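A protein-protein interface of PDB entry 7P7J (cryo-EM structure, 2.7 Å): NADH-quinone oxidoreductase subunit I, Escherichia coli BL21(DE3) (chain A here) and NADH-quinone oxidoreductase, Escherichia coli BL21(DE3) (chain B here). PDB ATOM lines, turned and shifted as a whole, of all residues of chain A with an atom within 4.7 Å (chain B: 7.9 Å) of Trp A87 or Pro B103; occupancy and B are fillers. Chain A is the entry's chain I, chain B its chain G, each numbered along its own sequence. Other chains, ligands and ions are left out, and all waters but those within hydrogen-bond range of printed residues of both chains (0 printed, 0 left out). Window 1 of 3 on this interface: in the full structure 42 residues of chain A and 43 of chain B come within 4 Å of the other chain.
The side-chain carboxylate of Asp B101 lies within hydrogen-bond range of the backbone NH of Met A156.
O of Ser B211 sits at hydrogen-bond distance from NZ of Lys A79, at 2.6 Å.
NE of Arg B216 sits at hydrogen-bond distance from O of Cys A63 (2.9 Å).
The backbone carbonyl oxygen (O) of Val B104 lies close to the side-chain sulfur (SD) of Met A156, 3.4 Å away.
The backbone carbonyl oxygen (O) of Pro B103 is in hydrogen-bond range of the guanidinium group (NH2) of Arg B216, at 2.6 Å.
The backbone NH (N) of Glu B107 sits close to the side-chain sulfur (SG) of Cys B105.
The guanidinium group (NH1) of Arg B149 lies within salt-bridge range of the side-chain carboxylate (OE1) of Glu B106 (3.9 Å).
The backbone carbonyl oxygen (O) of Gly B108 sits close to the guanidinium group (NH1) of Arg B216.
OH of Tyr B214 sits at hydrogen-bond distance from NH1 of Arg B216.
The side-chain hydroxyl (OH) of Tyr A151 is in hydrogen-bond range of the backbone NH (N) of Trp A87, 2.6 Å away.
Among the printed residues, merely in contact across the chains: Cys A63 with Pro B103 (3.3 Å), Trp A87 with Val B104 (3.3 Å), Tyr A151 with Val B104 (3.4 Å), Trp A87 with Glu B106 (3.4 Å), Phe A150 with His B100 (3.5 Å), Pro A110 with Pro B103 (3.6 Å), Met A156 with Arg B149 (3.6 Å), Val A61 with Val B104 (3.6 Å), Trp A87 with Pro B103 (3.6 Å), Lys A79 with Tyr B214 (3.6 Å), Phe A150 with Val B104 (3.7 Å), Phe A150 with Pro B103 (3.7 Å), Val A61 with Pro B103 (3.9 Å), Trp A87 with Cys B105 (3.9 Å) and Trp A87 with Tyr B214 (3.98 Å).
Of the printed residues of chain B, Trp A87 touches Pro B103, Val B104, Cys B105, Glu B106 and Tyr B214.
Of the printed residues of chain A, Pro B103 touches Val A61 (3.9 Å), Cys A63 (3.3 Å), Trp A87 (3.6 Å), Pro A110 (3.6 Å) and Phe A150 (3.7 Å).
Printed residues of chain B within 4 Å of Cys A63: Pro B103 and Arg B216.
Printed residues of chain A within 4 Å of Val B104: Val A61 (3.6 Å), Trp A87 (3.3 Å), Phe A150 (3.7 Å), Tyr A151 (3.4 Å) and Met A156 (3.4 Å).
Of the printed residues of chain A, Arg B149 touches Met A156 (3.6 Å).
Glu A81 touches none of the printed residues of chain B.
The nearest printed residue of chain B that does not touch Tyr A151 is Asp B101 (6.9 Å).
Hydrophobic or aromatic side chains of chain B within 4 Å of the printed part of chain A: His B100, Pro B103, Val B104 and Tyr B214.
Along chain B the printed residues that touch a printed residue of chain A span positions 100 to 216.
Along chain A the printed residues that touch a printed residue of chain B span positions 61 to 156.
Among the printed residues, no Asp or Glu carboxylate lies within 4 Å of a Lys or Arg side-chain nitrogen of the other chain.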
ATOM      1  N   CYS A  60     -17.643  35.705  -7.010  1.00  0.00           N
ATOM      2  CA  CYS A  60     -19.034  35.734  -6.584  1.00  0.00           C
ATOM      3  C   CYS A  60     -19.890  34.865  -7.488  1.00  0.00           C
ATOM      4  O   CYS A  60     -19.886  35.020  -8.711  1.00  0.00           O
ATOM      5  CB  CYS A  60     -19.569  37.160  -6.569  1.00  0.00           C
ATOM      6  SG  CYS A  60     -21.308  37.250  -6.117  1.00  0.00           S
ATOM      7  N   VAL A  61     -20.624  33.943  -6.872  1.00  0.00           N
ATOM      8  CA  VAL A  61     -21.540  33.074  -7.586  1.00  0.00           C
ATOM      9  C   VAL A  61     -22.976  33.564  -7.484  1.00  0.00           C
ATOM     10  O   VAL A  61     -23.897  32.840  -7.863  1.00  0.00           O
ATOM     11  CB  VAL A  61     -21.417  31.630  -7.088  1.00  0.00           C
ATOM     12  CG1 VAL A  61     -20.004  31.133  -7.274  1.00  0.00           C
ATOM     13  CG2 VAL A  61     -21.840  31.528  -5.634  1.00  0.00           C
ATOM     14  N   ALA A  62     -23.182  34.776  -6.967  1.00  0.00           N
ATOM     15  CA  ALA A  62     -24.494  35.415  -6.848  1.00  0.00           C
ATOM     16  C   ALA A  62     -25.485  34.538  -6.089  1.00  0.00           C
ATOM     17  O   ALA A  62     -26.631  34.348  -6.495  1.00  0.00           O
ATOM     18  CB  ALA A  62     -25.040  35.807  -8.216  1.00  0.00           C
ATOM     19  N   CYS A  63     -25.022  33.990  -4.973  1.00  0.00           N
ATOM     20  CA  CYS A  63     -25.837  33.078  -4.190  1.00  0.00           C
ATOM     21  C   CYS A  63     -26.764  33.786  -3.213  1.00  0.00           C
ATOM     22  O   CYS A  63     -27.608  33.120  -2.606  1.00  0.00           O
ATOM     23  CB  CYS A  63     -24.928  32.114  -3.440  1.00  0.00           C
ATOM     24  SG  CYS A  63     -24.209  32.780  -1.953  1.00  0.00           S
ATOM     25  N   LYS A  79     -28.603  37.160  -9.862  1.00  0.00           N
ATOM     26  CA  LYS A  79     -27.868  36.055 -10.451  1.00  0.00           C
ATOM     27  C   LYS A  79     -27.990  36.070 -11.967  1.00  0.00           C
ATOM     28  O   LYS A  79     -29.075  36.275 -12.517  1.00  0.00           O
ATOM     29  CB  LYS A  79     -28.379  34.729  -9.887  1.00  0.00           C
ATOM     30  CG  LYS A  79     -27.800  33.490 -10.536  1.00  0.00           C
ATOM     31  CD  LYS A  79     -28.854  32.753 -11.330  1.00  0.00           C
ATOM     32  CE  LYS A  79     -28.246  31.718 -12.242  1.00  0.00           C
ATOM     33  NZ  LYS A  79     -29.285  31.003 -13.018  1.00  0.00           N
ATOM     34  N   ALA A  80     -26.865  35.858 -12.642  1.00  0.00           N
ATOM     35  CA  ALA A  80     -26.823  35.653 -14.076  1.00  0.00           C
ATOM     36  C   ALA A  80     -25.909  34.472 -14.356  1.00  0.00           C
ATOM     37  O   ALA A  80     -25.083  34.089 -13.526  1.00  0.00           O
ATOM     38  CB  ALA A  80     -26.334  36.902 -14.817  1.00  0.00           C
ATOM     39  N   GLU A  81     -26.076  33.880 -15.529  1.00  0.00           N
ATOM     40  CA  GLU A  81     -25.340  32.682 -15.893  1.00  0.00           C
ATOM     41  C   GLU A  81     -24.682  32.877 -17.248  1.00  0.00           C
ATOM     42  O   GLU A  81     -25.299  33.410 -18.174  1.00  0.00           O
ATOM     43  CB  GLU A  81     -26.266  31.470 -15.930  1.00  0.00           C
ATOM     44  CG  GLU A  81     -25.567  30.149 -15.741  1.00  0.00           C
ATOM     45  CD  GLU A  81     -26.536  29.023 -15.470  1.00  0.00           C
ATOM     46  OE1 GLU A  81     -27.716  29.314 -15.192  1.00  0.00           O
ATOM     47  OE2 GLU A  81     -26.122  27.847 -15.538  1.00  0.00           O
ATOM     48  N   GLY A  85     -22.109  27.880 -17.888  1.00  0.00           N
ATOM     49  CA  GLY A  85     -23.003  27.496 -16.820  1.00  0.00           C
ATOM     50  C   GLY A  85     -22.575  27.974 -15.451  1.00  0.00           C
ATOM     51  O   GLY A  85     -23.137  27.535 -14.443  1.00  0.00           O
ATOM     52  N   ARG A  86     -21.591  28.863 -15.385  1.00  0.00           N
ATOM     53  CA  ARG A  86     -21.170  29.397 -14.101  1.00  0.00           C
ATOM     54  C   ARG A  86     -22.050  30.577 -13.713  1.00  0.00           C
ATOM     55  O   ARG A  86     -22.532  31.333 -14.561  1.00  0.00           O
ATOM     56  CB  ARG A  86     -19.689  29.794 -14.117  1.00  0.00           C
ATOM     57  CG  ARG A  86     -19.363  31.207 -14.541  1.00  0.00           C
ATOM     58  CD  ARG A  86     -17.874  31.463 -14.440  1.00  0.00           C
ATOM     59  NE  ARG A  86     -17.430  31.640 -13.064  1.00  0.00           N
ATOM     60  CZ  ARG A  86     -16.218  31.331 -12.624  1.00  0.00           C
ATOM     61  NH1 ARG A  86     -15.318  30.773 -13.415  1.00  0.00           N
ATOM     62  NH2 ARG A  86     -15.901  31.588 -11.358  1.00  0.00           N
ATOM     63  N   TRP A  87     -22.290  30.699 -12.416  1.00  0.00           N
ATOM     64  CA  TRP A  87     -23.113  31.766 -11.878  1.00  0.00           C
ATOM     65  C   TRP A  87     -22.232  32.963 -11.555  1.00  0.00           C
ATOM     66  O   TRP A  87     -21.086  32.808 -11.130  1.00  0.00           O
ATOM     67  CB  TRP A  87     -23.838  31.311 -10.614  1.00  0.00           C
ATOM     68  CG  TRP A  87     -24.929  30.297 -10.778  1.00  0.00           C
ATOM     69  CD1 TRP A  87     -25.056  29.371 -11.765  1.00  0.00           C
ATOM     70  CD2 TRP A  87     -26.035  30.095  -9.894  1.00  0.00           C
ATOM     71  NE1 TRP A  87     -26.180  28.612 -11.560  1.00  0.00           N
ATOM     72  CE2 TRP A  87     -26.802  29.041 -10.418  1.00  0.00           C
ATOM     73  CE3 TRP A  87     -26.460  30.713  -8.715  1.00  0.00           C
ATOM     74  CZ2 TRP A  87     -27.963  28.587  -9.802  1.00  0.00           C
ATOM     75  CZ3 TRP A  87     -27.614  30.264  -8.108  1.00  0.00           C
ATOM     76  CH2 TRP A  87     -28.351  29.212  -8.651  1.00  0.00           C
ATOM     77  N   TYR A  88     -22.770  34.157 -11.764  1.00  0.00           N
ATOM     78  CA  TYR A  88     -22.057  35.389 -11.467  1.00  0.00           C
ATOM     79  C   TYR A  88     -23.092  36.460 -11.167  1.00  0.00           C
ATOM     80  O   TYR A  88     -24.278  36.272 -11.455  1.00  0.00           O
ATOM     81  CB  TYR A  88     -21.129  35.791 -12.627  1.00  0.00           C
ATOM     82  CG  TYR A  88     -21.815  36.327 -13.855  1.00  0.00           C
ATOM     83  CD1 TYR A  88     -22.391  35.471 -14.776  1.00  0.00           C
ATOM     84  CD2 TYR A  88     -21.867  37.689 -14.107  1.00  0.00           C
ATOM     85  CE1 TYR A  88     -23.015  35.953 -15.901  1.00  0.00           C
ATOM     86  CE2 TYR A  88     -22.489  38.183 -15.229  1.00  0.00           C
ATOM     87  CZ  TYR A  88     -23.060  37.309 -16.125  1.00  0.00           C
ATOM     88  OH  TYR A  88     -23.682  37.790 -17.250  1.00  0.00           O
ATOM     89  N   PRO A 110     -19.858  31.944   1.119  1.00  0.00           N
ATOM     90  CA  PRO A 110     -19.274  30.610   0.958  1.00  0.00           C
ATOM     91  C   PRO A 110     -18.217  30.513  -0.129  1.00  0.00           C
ATOM     92  O   PRO A 110     -17.678  29.424  -0.341  1.00  0.00           O
ATOM     93  CB  PRO A 110     -20.502  29.768   0.596  1.00  0.00           C
ATOM     94  CG  PRO A 110     -21.373  30.711  -0.137  1.00  0.00           C
ATOM     95  CD  PRO A 110     -21.127  32.084   0.388  1.00  0.00           C
ATOM     96  N   PHE A 150     -14.170  28.359  -5.157  1.00  0.00           N
ATOM     97  CA  PHE A 150     -15.390  27.611  -4.875  1.00  0.00           C
ATOM     98  C   PHE A 150     -15.715  26.635  -5.994  1.00  0.00           C
ATOM     99  O   PHE A 150     -16.158  25.510  -5.734  1.00  0.00           O
ATOM    100  CB  PHE A 150     -16.564  28.563  -4.651  1.00  0.00           C
ATOM    101  CG  PHE A 150     -17.902  27.879  -4.653  1.00  0.00           C
ATOM    102  CD1 PHE A 150     -18.298  27.108  -3.576  1.00  0.00           C
ATOM    103  CD2 PHE A 150     -18.754  27.989  -5.737  1.00  0.00           C
ATOM    104  CE1 PHE A 150     -19.518  26.471  -3.576  1.00  0.00           C
ATOM    105  CE2 PHE A 150     -19.971  27.352  -5.741  1.00  0.00           C
ATOM    106  CZ  PHE A 150     -20.353  26.591  -4.660  1.00  0.00           C
ATOM    107  N   TYR A 151     -15.498  27.041  -7.243  1.00  0.00           N
ATOM    108  CA  TYR A 151     -15.858  26.206  -8.379  1.00  0.00           C
ATOM    109  C   TYR A 151     -14.939  25.008  -8.552  1.00  0.00           C
ATOM    110  O   TYR A 151     -15.276  24.100  -9.316  1.00  0.00           O
ATOM    111  CB  TYR A 151     -15.880  27.050  -9.648  1.00  0.00           C
ATOM    112  CG  TYR A 151     -17.232  27.660  -9.910  1.00  0.00           C
ATOM    113  CD1 TYR A 151     -18.348  26.858 -10.091  1.00  0.00           C
ATOM    114  CD2 TYR A 151     -17.398  29.034  -9.963  1.00  0.00           C
ATOM    115  CE1 TYR A 151     -19.586  27.404 -10.326  1.00  0.00           C
ATOM    116  CE2 TYR A 151     -18.636  29.590 -10.199  1.00  0.00           C
ATOM    117  CZ  TYR A 151     -19.726  28.769 -10.378  1.00  0.00           C
ATOM    118  OH  TYR A 151     -20.963  29.317 -10.613  1.00  0.00           O
ATOM    119  N   MET A 156     -21.179  21.491 -10.054  1.00  0.00           N
ATOM    120  CA  MET A 156     -21.638  21.905 -11.373  1.00  0.00           C
ATOM    121  C   MET A 156     -20.484  21.916 -12.364  1.00  0.00           C
ATOM    122  O   MET A 156     -19.342  22.229 -12.021  1.00  0.00           O
ATOM    123  CB  MET A 156     -22.269  23.295 -11.333  1.00  0.00           C
ATOM    124  CG  MET A 156     -23.717  23.336 -10.896  1.00  0.00           C
ATOM    125  SD  MET A 156     -24.517  24.914 -11.275  1.00  0.00           S
ATOM    126  CE  MET A 156     -23.128  26.047 -11.302  1.00  0.00           C
ATOM    127  N   PRO B  99     -23.029  16.784  -3.840  1.00  0.00           N
ATOM    128  CA  PRO B  99     -22.105  17.813  -4.322  1.00  0.00           C
ATOM    129  C   PRO B  99     -22.116  19.056  -3.450  1.00  0.00           C
ATOM    130  O   PRO B  99     -23.126  19.411  -2.839  1.00  0.00           O
ATOM    131  CB  PRO B  99     -22.634  18.124  -5.724  1.00  0.00           C
ATOM    132  CG  PRO B  99     -24.068  17.804  -5.642  1.00  0.00           C
ATOM    133  CD  PRO B  99     -24.165  16.606  -4.756  1.00  0.00           C
ATOM    134  N   HIS B 100     -20.968  19.732  -3.426  1.00  0.00           N
ATOM    135  CA  HIS B 100     -20.774  20.985  -2.697  1.00  0.00           C
ATOM    136  C   HIS B 100     -21.414  22.125  -3.493  1.00  0.00           C
ATOM    137  O   HIS B 100     -20.753  23.030  -4.002  1.00  0.00           O
ATOM    138  CB  HIS B 100     -19.285  21.216  -2.472  1.00  0.00           C
ATOM    139  CG  HIS B 100     -18.972  22.290  -1.479  1.00  0.00           C
ATOM    140  ND1 HIS B 100     -18.720  22.023  -0.152  1.00  0.00           N
ATOM    141  CD2 HIS B 100     -18.850  23.629  -1.624  1.00  0.00           C
ATOM    142  CE1 HIS B 100     -18.471  23.154   0.481  1.00  0.00           C
ATOM    143  NE2 HIS B 100     -18.542  24.143  -0.390  1.00  0.00           N
ATOM    144  N   ASP B 101     -22.741  22.080  -3.580  1.00  0.00           N
ATOM    145  CA  ASP B 101     -23.442  22.807  -4.623  1.00  0.00           C
ATOM    146  C   ASP B 101     -24.433  23.849  -4.136  1.00  0.00           C
ATOM    147  O   ASP B 101     -24.955  24.588  -4.975  1.00  0.00           O
ATOM    148  CB  ASP B 101     -24.191  21.825  -5.536  1.00  0.00           C
ATOM    149  CG  ASP B 101     -23.512  21.624  -6.857  1.00  0.00           C
ATOM    150  OD1 ASP B 101     -22.361  22.068  -7.008  1.00  0.00           O
ATOM    151  OD2 ASP B 101     -24.137  21.024  -7.751  1.00  0.00           O
ATOM    152  N   CYS B 102     -24.690  23.945  -2.831  1.00  0.00           N
ATOM    153  CA  CYS B 102     -25.750  24.813  -2.309  1.00  0.00           C
ATOM    154  C   CYS B 102     -25.701  26.276  -2.756  1.00  0.00           C
ATOM    155  O   CYS B 102     -26.778  26.822  -3.047  1.00  0.00           O
ATOM    156  CB  CYS B 102     -25.775  24.754  -0.774  1.00  0.00           C
ATOM    157  SG  CYS B 102     -26.137  23.161  -0.044  1.00  0.00           S
ATOM    158  N   PRO B 103     -24.551  26.973  -2.814  1.00  0.00           N
ATOM    159  CA  PRO B 103     -24.580  28.346  -3.347  1.00  0.00           C
ATOM    160  C   PRO B 103     -25.004  28.446  -4.802  1.00  0.00           C
ATOM    161  O   PRO B 103     -25.627  29.441  -5.181  1.00  0.00           O
ATOM    162  CB  PRO B 103     -23.134  28.822  -3.158  1.00  0.00           C
ATOM    163  CG  PRO B 103     -22.606  27.983  -2.096  1.00  0.00           C
ATOM    164  CD  PRO B 103     -23.201  26.660  -2.305  1.00  0.00           C
ATOM    165  N   VAL B 104     -24.701  27.445  -5.623  1.00  0.00           N
ATOM    166  CA  VAL B 104     -24.989  27.509  -7.050  1.00  0.00           C
ATOM    167  C   VAL B 104     -26.112  26.548  -7.407  1.00  0.00           C
ATOM    168  O   VAL B 104     -26.192  26.062  -8.538  1.00  0.00           O
ATOM    169  CB  VAL B 104     -23.736  27.204  -7.886  1.00  0.00           C
ATOM    170  CG1 VAL B 104     -22.840  28.404  -7.947  1.00  0.00           C
ATOM    171  CG2 VAL B 104     -22.999  26.012  -7.320  1.00  0.00           C
ATOM    172  N   CYS B 105     -26.981  26.265  -6.450  1.00  0.00           N
ATOM    173  CA  CYS B 105     -28.103  25.364  -6.646  1.00  0.00           C
ATOM    174  C   CYS B 105     -29.395  26.140  -6.466  1.00  0.00           C
ATOM    175  O   CYS B 105     -29.530  26.923  -5.522  1.00  0.00           O
ATOM    176  CB  CYS B 105     -28.029  24.202  -5.668  1.00  0.00           C
ATOM    177  SG  CYS B 105     -29.388  23.059  -5.640  1.00  0.00           S
ATOM    178  N   GLU B 106     -30.344  25.921  -7.372  1.00  0.00           N
ATOM    179  CA  GLU B 106     -31.595  26.662  -7.336  1.00  0.00           C
ATOM    180  C   GLU B 106     -32.524  26.213  -6.221  1.00  0.00           C
ATOM    181  O   GLU B 106     -33.517  26.895  -5.959  1.00  0.00           O
ATOM    182  CB  GLU B 106     -32.314  26.544  -8.677  1.00  0.00           C
ATOM    183  CG  GLU B 106     -31.690  27.366  -9.777  1.00  0.00           C
ATOM    184  CD  GLU B 106     -30.760  26.556 -10.650  1.00  0.00           C
ATOM    185  OE1 GLU B 106     -30.444  25.405 -10.285  1.00  0.00           O
ATOM    186  OE2 GLU B 106     -30.342  27.071 -11.705  1.00  0.00           O
ATOM    187  N   GLU B 107     -32.245  25.096  -5.564  1.00  0.00           N
ATOM    188  CA  GLU B 107     -33.092  24.650  -4.472  1.00  0.00           C
ATOM    189  C   GLU B 107     -32.659  25.186  -3.117  1.00  0.00           C
ATOM    190  O   GLU B 107     -33.365  24.952  -2.136  1.00  0.00           O
ATOM    191  CB  GLU B 107     -33.139  23.125  -4.427  1.00  0.00           C
ATOM    192  CG  GLU B 107     -34.288  22.561  -5.229  1.00  0.00           C
ATOM    193  CD  GLU B 107     -35.529  22.351  -4.406  1.00  0.00           C
ATOM    194  OE1 GLU B 107     -35.396  22.173  -3.184  1.00  0.00           O
ATOM    195  OE2 GLU B 107     -36.637  22.353  -4.980  1.00  0.00           O
ATOM    196  N   GLY B 108     -31.539  25.900  -3.043  1.00  0.00           N
ATOM    197  CA  GLY B 108     -31.066  26.476  -1.798  1.00  0.00           C
ATOM    198  C   GLY B 108     -32.042  27.436  -1.154  1.00  0.00           C
ATOM    199  O   GLY B 108     -32.562  28.340  -1.811  1.00  0.00           O
ATOM    200  N   GLN B 114     -31.747  20.112   2.673  1.00  0.00           N
ATOM    201  CA  GLN B 114     -31.123  21.055   3.597  1.00  0.00           C
ATOM    202  C   GLN B 114     -31.852  21.082   4.933  1.00  0.00           C
ATOM    203  O   GLN B 114     -31.221  21.052   5.999  1.00  0.00           O
ATOM    204  CB  GLN B 114     -31.106  22.455   2.989  1.00  0.00           C
ATOM    205  CG  GLN B 114     -30.020  22.715   1.980  1.00  0.00           C
ATOM    206  CD  GLN B 114     -29.911  24.179   1.638  1.00  0.00           C
ATOM    207  OE1 GLN B 114     -30.918  24.850   1.427  1.00  0.00           O
ATOM    208  NE2 GLN B 114     -28.688  24.690   1.593  1.00  0.00           N
ATOM    209  N   ARG B 149     -27.189  15.873  -7.395  1.00  0.00           N
ATOM    210  CA  ARG B 149     -27.863  16.222  -6.156  1.00  0.00           C
ATOM    211  C   ARG B 149     -28.865  15.176  -5.694  1.00  0.00           C
ATOM    212  O   ARG B 149     -29.508  15.378  -4.664  1.00  0.00           O
ATOM    213  CB  ARG B 149     -28.564  17.571  -6.315  1.00  0.00           C
ATOM    214  CG  ARG B 149     -27.610  18.715  -6.538  1.00  0.00           C
ATOM    215  CD  ARG B 149     -28.286  19.895  -7.190  1.00  0.00           C
ATOM    216  NE  ARG B 149     -27.310  20.863  -7.668  1.00  0.00           N
ATOM    217  CZ  ARG B 149     -27.595  21.893  -8.449  1.00  0.00           C
ATOM    218  NH1 ARG B 149     -28.828  22.127  -8.859  1.00  0.00           N
ATOM    219  NH2 ARG B 149     -26.615  22.701  -8.839  1.00  0.00           N
ATOM    220  N   SER B 211     -34.967  29.485 -13.191  1.00  0.00           N
ATOM    221  CA  SER B 211     -33.509  29.469 -13.134  1.00  0.00           C
ATOM    222  C   SER B 211     -32.876  30.509 -14.043  1.00  0.00           C
ATOM    223  O   SER B 211     -31.712  30.864 -13.837  1.00  0.00           O
ATOM    224  CB  SER B 211     -32.975  28.086 -13.499  1.00  0.00           C
ATOM    225  OG  SER B 211     -31.576  28.117 -13.693  1.00  0.00           O
ATOM    226  N   TYR B 214     -33.167  33.818 -11.548  1.00  0.00           N
ATOM    227  CA  TYR B 214     -33.271  33.150 -10.260  1.00  0.00           C
ATOM    228  C   TYR B 214     -33.140  34.127  -9.103  1.00  0.00           C
ATOM    229  O   TYR B 214     -32.318  35.045  -9.127  1.00  0.00           O
ATOM    230  CB  TYR B 214     -32.219  32.051 -10.117  1.00  0.00           C
ATOM    231  CG  TYR B 214     -32.312  31.332  -8.789  1.00  0.00           C
ATOM    232  CD1 TYR B 214     -33.325  30.420  -8.549  1.00  0.00           C
ATOM    233  CD2 TYR B 214     -31.412  31.596  -7.767  1.00  0.00           C
ATOM    234  CE1 TYR B 214     -33.435  29.783  -7.337  1.00  0.00           C
ATOM    235  CE2 TYR B 214     -31.512  30.959  -6.551  1.00  0.00           C
ATOM    236  CZ  TYR B 214     -32.523  30.051  -6.344  1.00  0.00           C
ATOM    237  OH  TYR B 214     -32.631  29.410  -5.135  1.00  0.00           O
ATOM    238  N   ASN B 215     -33.961  33.910  -8.082  1.00  0.00           N
ATOM    239  CA  ASN B 215     -33.796  34.535  -6.783  1.00  0.00           C
ATOM    240  C   ASN B 215     -34.227  33.534  -5.724  1.00  0.00           C
ATOM    241  O   ASN B 215     -35.013  32.622  -5.991  1.00  0.00           O
ATOM    242  CB  ASN B 215     -34.605  35.831  -6.662  1.00  0.00           C
ATOM    243  CG  ASN B 215     -36.083  35.577  -6.540  1.00  0.00           C
ATOM    244  OD1 ASN B 215     -36.659  34.836  -7.328  1.00  0.00           O
ATOM    245  ND2 ASN B 215     -36.707  36.180  -5.542  1.00  0.00           N
ATOM    246  N   ARG B 216     -33.693  33.700  -4.523  1.00  0.00           N
ATOM    247  CA  ARG B 216     -33.978  32.765  -3.449  1.00  0.00           C
ATOM    248  C   ARG B 216     -35.365  33.012  -2.869  1.00  0.00           C
ATOM    249  O   ARG B 216     -35.969  34.067  -3.067  1.00  0.00           O
ATOM    250  CB  ARG B 216     -32.919  32.871  -2.361  1.00  0.00           C
ATOM    251  CG  ARG B 216     -31.508  32.724  -2.878  1.00  0.00           C
ATOM    252  CD  ARG B 216     -31.062  31.290  -2.835  1.00  0.00           C
ATOM    253  NE  ARG B 216     -29.671  31.144  -3.234  1.00  0.00           N
ATOM    254  CZ  ARG B 216     -29.131  30.011  -3.649  1.00  0.00           C
ATOM    255  NH1 ARG B 216     -29.849  28.911  -3.765  1.00  0.00           N
ATOM    256  NH2 ARG B 216     -27.842  29.984  -3.962  1.00  0.00           N
